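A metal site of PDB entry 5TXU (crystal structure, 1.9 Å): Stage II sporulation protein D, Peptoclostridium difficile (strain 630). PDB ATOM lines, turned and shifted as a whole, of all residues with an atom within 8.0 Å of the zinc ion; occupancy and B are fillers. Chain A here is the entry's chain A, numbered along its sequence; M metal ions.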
ATOM      1  N   TYR A  78     -18.849   9.268  20.360  1.00  0.00           N
ATOM      2  CA  TYR A  78     -18.868   8.755  21.726  1.00  0.00           C
ATOM      3  C   TYR A  78     -20.217   9.048  22.376  1.00  0.00           C
ATOM      4  O   TYR A  78     -20.638  10.189  22.469  1.00  0.00           O
ATOM      5  CB  TYR A  78     -17.741   9.379  22.550  1.00  0.00           C
ATOM      6  CG  TYR A  78     -17.736   8.978  24.019  1.00  0.00           C
ATOM      7  CD1 TYR A  78     -17.327   7.697  24.408  1.00  0.00           C
ATOM      8  CD2 TYR A  78     -18.094   9.882  25.018  1.00  0.00           C
ATOM      9  CE1 TYR A  78     -17.303   7.328  25.754  1.00  0.00           C
ATOM     10  CE2 TYR A  78     -18.071   9.523  26.366  1.00  0.00           C
ATOM     11  CZ  TYR A  78     -17.683   8.245  26.734  1.00  0.00           C
ATOM     12  OH  TYR A  78     -17.666   7.891  28.061  1.00  0.00           O
ATOM     13  N   HIS A  80     -22.052   9.589  25.417  1.00  0.00           N
ATOM     14  CA  HIS A  80     -21.737   9.980  26.805  1.00  0.00           C
ATOM     15  C   HIS A  80     -22.573   9.275  27.885  1.00  0.00           C
ATOM     16  O   HIS A  80     -22.215   9.318  29.063  1.00  0.00           O
ATOM     17  CB  HIS A  80     -21.817  11.503  26.979  1.00  0.00           C
ATOM     18  CG  HIS A  80     -23.212  12.028  27.131  1.00  0.00           C
ATOM     19  ND1 HIS A  80     -24.079  12.154  26.075  1.00  0.00           N
ATOM     20  CD2 HIS A  80     -23.872  12.471  28.221  1.00  0.00           C
ATOM     21  CE1 HIS A  80     -25.234  12.648  26.507  1.00  0.00           C
ATOM     22  NE2 HIS A  80     -25.129  12.847  27.816  1.00  0.00           N
ATOM     23  N   TYR A  93     -25.289  11.551  11.522  1.00  0.00           N
ATOM     24  CA  TYR A  93     -24.871  12.246  12.735  1.00  0.00           C
ATOM     25  C   TYR A  93     -25.425  13.657  12.715  1.00  0.00           C
ATOM     26  O   TYR A  93     -26.054  14.080  13.691  1.00  0.00           O
ATOM     27  CB  TYR A  93     -23.324  12.276  12.889  1.00  0.00           C
ATOM     28  CG  TYR A  93     -22.876  13.256  13.964  1.00  0.00           C
ATOM     29  CD1 TYR A  93     -23.112  13.006  15.292  1.00  0.00           C
ATOM     30  CD2 TYR A  93     -22.225  14.442  13.624  1.00  0.00           C
ATOM     31  CE1 TYR A  93     -22.714  13.900  16.276  1.00  0.00           C
ATOM     32  CE2 TYR A  93     -21.820  15.347  14.605  1.00  0.00           C
ATOM     33  CZ  TYR A  93     -22.075  15.074  15.934  1.00  0.00           C
ATOM     34  OH  TYR A  93     -21.705  15.974  16.919  1.00  0.00           O
ATOM     35  N   TYR A 121     -17.925  21.724  12.822  1.00  0.00           N
ATOM     36  CA  TYR A 121     -17.459  21.354  14.172  1.00  0.00           C
ATOM     37  C   TYR A 121     -16.724  20.017  14.146  1.00  0.00           C
ATOM     38  O   TYR A 121     -15.636  19.858  14.722  1.00  0.00           O
ATOM     39  CB  TYR A 121     -18.633  21.319  15.149  1.00  0.00           C
ATOM     40  CG  TYR A 121     -18.205  21.134  16.573  1.00  0.00           C
ATOM     41  CD1 TYR A 121     -17.864  22.233  17.366  1.00  0.00           C
ATOM     42  CD2 TYR A 121     -18.152  19.871  17.142  1.00  0.00           C
ATOM     43  CE1 TYR A 121     -17.462  22.079  18.694  1.00  0.00           C
ATOM     44  CE2 TYR A 121     -17.748  19.697  18.465  1.00  0.00           C
ATOM     45  CZ  TYR A 121     -17.405  20.803  19.231  1.00  0.00           C
ATOM     46  OH  TYR A 121     -17.028  20.643  20.527  1.00  0.00           O
ATOM     47  N   LYS A 125     -12.708  19.507  14.810  1.00  0.00           N
ATOM     48  CA  LYS A 125     -12.309  18.494  15.791  1.00  0.00           C
ATOM     49  C   LYS A 125     -11.351  17.431  15.216  1.00  0.00           C
ATOM     50  O   LYS A 125     -10.422  17.009  15.901  1.00  0.00           O
ATOM     51  CB  LYS A 125     -13.538  17.823  16.417  1.00  0.00           C
ATOM     52  CG  LYS A 125     -13.964  18.294  17.801  1.00  0.00           C
ATOM     53  CD  LYS A 125     -13.708  19.761  18.150  1.00  0.00           C
ATOM     54  CE  LYS A 125     -13.816  19.960  19.654  1.00  0.00           C
ATOM     55  NZ  LYS A 125     -13.245  21.261  20.114  1.00  0.00           N
ATOM     56  N   SER A 131      -9.565  15.080  22.612  1.00  0.00           N
ATOM     57  CA  SER A 131      -9.921  15.424  23.996  1.00  0.00           C
ATOM     58  C   SER A 131      -9.723  14.233  24.932  1.00  0.00           C
ATOM     59  O   SER A 131      -9.726  13.077  24.489  1.00  0.00           O
ATOM     60  CB  SER A 131     -11.365  15.908  24.078  1.00  0.00           C
ATOM     61  OG  SER A 131     -12.266  14.893  23.646  1.00  0.00           O
ATOM     62  N   LYS A 133     -11.852  13.439  27.363  1.00  0.00           N
ATOM     63  CA  LYS A 133     -13.167  12.792  27.554  1.00  0.00           C
ATOM     64  C   LYS A 133     -13.398  11.605  26.620  1.00  0.00           C
ATOM     65  O   LYS A 133     -14.037  10.628  27.004  1.00  0.00           O
ATOM     66  CB  LYS A 133     -14.335  13.771  27.355  1.00  0.00           C
ATOM     67  CG  LYS A 133     -14.886  14.436  28.607  1.00  0.00           C
ATOM     68  CD  LYS A 133     -14.061  15.590  29.114  1.00  0.00           C
ATOM     69  CE  LYS A 133     -14.807  16.307  30.225  1.00  0.00           C
ATOM     70  NZ  LYS A 133     -14.115  17.552  30.675  1.00  0.00           N
ATOM     71  N   HIS A 134     -12.905  11.716  25.392  1.00  0.00           N
ATOM     72  CA  HIS A 134     -13.088  10.662  24.405  1.00  0.00           C
ATOM     73  C   HIS A 134     -11.999  10.748  23.349  1.00  0.00           C
ATOM     74  O   HIS A 134     -12.218  11.206  22.222  1.00  0.00           O
ATOM     75  CB  HIS A 134     -14.507  10.742  23.781  1.00  0.00           C
ATOM     76  CG  HIS A 134     -14.890  12.111  23.297  1.00  0.00           C
ATOM     77  ND1 HIS A 134     -14.527  12.591  22.062  1.00  0.00           N
ATOM     78  CD2 HIS A 134     -15.599  13.094  23.893  1.00  0.00           C
ATOM     79  CE1 HIS A 134     -15.009  13.806  21.907  1.00  0.00           C
ATOM     80  NE2 HIS A 134     -15.671  14.134  22.997  1.00  0.00           N
ATOM     81  N   ALA A 137     -12.750   9.196  19.814  1.00  0.00           N
ATOM     82  CA  ALA A 137     -13.922   9.665  19.071  1.00  0.00           C
ATOM     83  C   ALA A 137     -13.750  11.139  18.762  1.00  0.00           C
ATOM     84  O   ALA A 137     -13.341  11.926  19.640  1.00  0.00           O
ATOM     85  CB  ALA A 137     -15.194   9.442  19.880  1.00  0.00           C
ATOM     86  N   VAL A 138     -14.091  11.523  17.545  1.00  0.00           N
ATOM     87  CA  VAL A 138     -13.971  12.929  17.151  1.00  0.00           C
ATOM     88  C   VAL A 138     -14.986  13.793  17.915  1.00  0.00           C
ATOM     89  O   VAL A 138     -14.684  14.926  18.299  1.00  0.00           O
ATOM     90  CB  VAL A 138     -14.084  13.106  15.614  1.00  0.00           C
ATOM     91  CG1 VAL A 138     -15.434  12.652  15.086  1.00  0.00           C
ATOM     92  CG2 VAL A 138     -13.813  14.557  15.238  1.00  0.00           C
ATOM     93  N   VAL A 139     -16.195  13.279  18.121  1.00  0.00           N
ATOM     94  CA  VAL A 139     -17.229  14.007  18.843  1.00  0.00           C
ATOM     95  C   VAL A 139     -17.978  13.093  19.800  1.00  0.00           C
ATOM     96  O   VAL A 139     -17.938  11.867  19.663  1.00  0.00           O
ATOM     97  CB  VAL A 139     -18.268  14.650  17.880  1.00  0.00           C
ATOM     98  CG1 VAL A 139     -17.616  15.742  17.035  1.00  0.00           C
ATOM     99  CG2 VAL A 139     -18.929  13.609  16.992  1.00  0.00           C
ATOM    100  N   CYS A 140     -18.654  13.710  20.765  1.00  0.00           N
ATOM    101  CA  CYS A 140     -19.516  12.962  21.672  1.00  0.00           C
ATOM    102  C   CYS A 140     -20.947  13.512  21.573  1.00  0.00           C
ATOM    103  O   CYS A 140     -21.210  14.526  20.904  1.00  0.00           O
ATOM    104  CB  CYS A 140     -19.014  13.005  23.127  1.00  0.00           C
ATOM    105  SG  CYS A 140     -19.168  14.609  23.952  1.00  0.00           S
ATOM    106  N   THR A 141     -21.851  12.835  22.255  1.00  0.00           N
ATOM    107  CA  THR A 141     -23.284  13.192  22.269  1.00  0.00           C
ATOM    108  C   THR A 141     -23.673  14.147  23.425  1.00  0.00           C
ATOM    109  O   THR A 141     -24.866  14.386  23.653  1.00  0.00           O
ATOM    110  CB  THR A 141     -24.128  11.902  22.348  1.00  0.00           C
ATOM    111  OG1 THR A 141     -23.755  11.162  23.513  1.00  0.00           O
ATOM    112  CG2 THR A 141     -23.872  11.031  21.119  1.00  0.00           C
ATOM    113  N   ASP A 142     -22.687  14.699  24.138  1.00  0.00           N
ATOM    114  CA  ASP A 142     -22.974  15.605  25.250  1.00  0.00           C
ATOM    115  C   ASP A 142     -22.940  17.059  24.791  1.00  0.00           C
ATOM    116  O   ASP A 142     -21.878  17.572  24.432  1.00  0.00           O
ATOM    117  CB  ASP A 142     -21.969  15.393  26.385  1.00  0.00           C
ATOM    118  CG  ASP A 142     -22.313  16.194  27.644  1.00  0.00           C
ATOM    119  OD1 ASP A 142     -23.307  16.953  27.623  1.00  0.00           O
ATOM    120  OD2 ASP A 142     -21.571  16.079  28.638  1.00  0.00           O
ATOM    121  N   TYR A 143     -24.100  17.719  24.841  1.00  0.00           N
ATOM    122  CA  TYR A 143     -24.209  19.138  24.455  1.00  0.00           C
ATOM    123  C   TYR A 143     -23.326  20.047  25.311  1.00  0.00           C
ATOM    124  O   TYR A 143     -22.974  21.144  24.893  1.00  0.00           O
ATOM    125  CB  TYR A 143     -25.659  19.626  24.515  1.00  0.00           C
ATOM    126  CG  TYR A 143     -26.189  19.855  25.907  1.00  0.00           C
ATOM    127  CD1 TYR A 143     -26.740  18.810  26.650  1.00  0.00           C
ATOM    128  CD2 TYR A 143     -26.137  21.125  26.497  1.00  0.00           C
ATOM    129  CE1 TYR A 143     -27.233  19.017  27.936  1.00  0.00           C
ATOM    130  CE2 TYR A 143     -26.623  21.345  27.779  1.00  0.00           C
ATOM    131  CZ  TYR A 143     -27.170  20.287  28.490  1.00  0.00           C
ATOM    132  OH  TYR A 143     -27.649  20.499  29.763  1.00  0.00           O
ATOM    133  N   LYS A 144     -23.007  19.600  26.526  1.00  0.00           N
ATOM    134  CA  LYS A 144     -22.105  20.355  27.425  1.00  0.00           C
ATOM    135  C   LYS A 144     -20.644  20.308  26.965  1.00  0.00           C
ATOM    136  O   LYS A 144     -19.838  21.122  27.414  1.00  0.00           O
ATOM    137  CB  LYS A 144     -22.173  19.789  28.856  1.00  0.00           C
ATOM    138  CG  LYS A 144     -23.547  19.831  29.508  1.00  0.00           C
ATOM    139  CD  LYS A 144     -23.491  19.142  30.863  1.00  0.00           C
ATOM    140  CE  LYS A 144     -24.876  19.032  31.491  1.00  0.00           C
ATOM    141  NZ  LYS A 144     -24.804  18.299  32.784  1.00  0.00           N
ATOM    142  N   HIS A 145     -20.304  19.362  26.086  1.00  0.00           N
ATOM    143  CA  HIS A 145     -18.912  19.211  25.633  1.00  0.00           C
ATOM    144  C   HIS A 145     -18.745  19.413  24.130  1.00  0.00           C
ATOM    145  O   HIS A 145     -17.840  20.136  23.685  1.00  0.00           O
ATOM    146  CB  HIS A 145     -18.359  17.842  26.029  1.00  0.00           C
ATOM    147  CG  HIS A 145     -16.883  17.726  25.858  1.00  0.00           C
ATOM    148  ND1 HIS A 145     -16.289  17.460  24.650  1.00  0.00           N
ATOM    149  CD2 HIS A 145     -15.863  17.900  26.733  1.00  0.00           C
ATOM    150  CE1 HIS A 145     -14.979  17.446  24.783  1.00  0.00           C
ATOM    151  NE2 HIS A 145     -14.686  17.721  26.039  1.00  0.00           N
ATOM    152  N   CYS A 146     -19.577  18.732  23.340  1.00  0.00           N
ATOM    153  CA  CYS A 146     -19.541  18.866  21.879  1.00  0.00           C
ATOM    154  C   CYS A 146     -20.826  19.554  21.420  1.00  0.00           C
ATOM    155  O   CYS A 146     -20.925  20.796  21.464  1.00  0.00           O
ATOM    156  CB  CYS A 146     -19.301  17.507  21.199  1.00  0.00           C
ATOM    157  SG  CYS A 146     -17.579  16.984  21.156  1.00  0.00           S
ATOM    158  N   GLN A 147     -21.814  18.782  20.966  1.00  0.00           N
ATOM    159  CA  GLN A 147     -23.084  19.368  20.548  1.00  0.00           C
ATOM    160  C   GLN A 147     -24.190  18.369  20.798  1.00  0.00           C
ATOM    161  O   GLN A 147     -23.948  17.180  20.985  1.00  0.00           O
ATOM    162  CB  GLN A 147     -23.040  19.906  19.094  1.00  0.00           C
ATOM    163  CG  GLN A 147     -22.394  18.985  18.089  1.00  0.00           C
ATOM    164  CD  GLN A 147     -22.066  19.620  16.715  1.00  0.00           C
ATOM    165  OE1 GLN A 147     -22.255  20.822  16.453  1.00  0.00           O
ATOM    166  NE2 GLN A 147     -21.567  18.794  15.843  1.00  0.00           N
HETATM  167 ZN    ZN M   1     -17.383  15.790  23.200  1.00  0.00          ZN
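The side-chain sulfur of Cys 140 lies close to the backbone NH of Asp 142 (3.5 Å).
The side-chain hydroxyl (OH) of Tyr 121 lies close to the side-chain sulfur (SG) of Cys 146 (3.8 Å).
The backbone carbonyl oxygen (O) of Ala 137 lies within hydrogen-bond range of a ring nitrogen (ND1) of His 134 (2.8 Å).
The side-chain hydroxyl (OH) of Tyr 121 lies within hydrogen-bond range of the backbone carbonyl oxygen (O) of His 145 (3.3 Å).
Within 4 Å of the zinc ion: His 134, Cys 140, His 145 and Cys 146.
Along chain A the residues within 4 Å of the zinc ion span positions 134 to 146.
The nearest printed residue that does not touch the zinc ion is Val 139 (4.4 Å).
SG of Cys 140 binds the zinc ion, at 2.3 Å.
SG of Cys 146 is bound to the zinc ion (2.4 Å).
The zinc ion is bound by NE2 of His 134 (2.4 Å).
The zinc ion is bound by ND1 of His 145 (2.5 Å).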
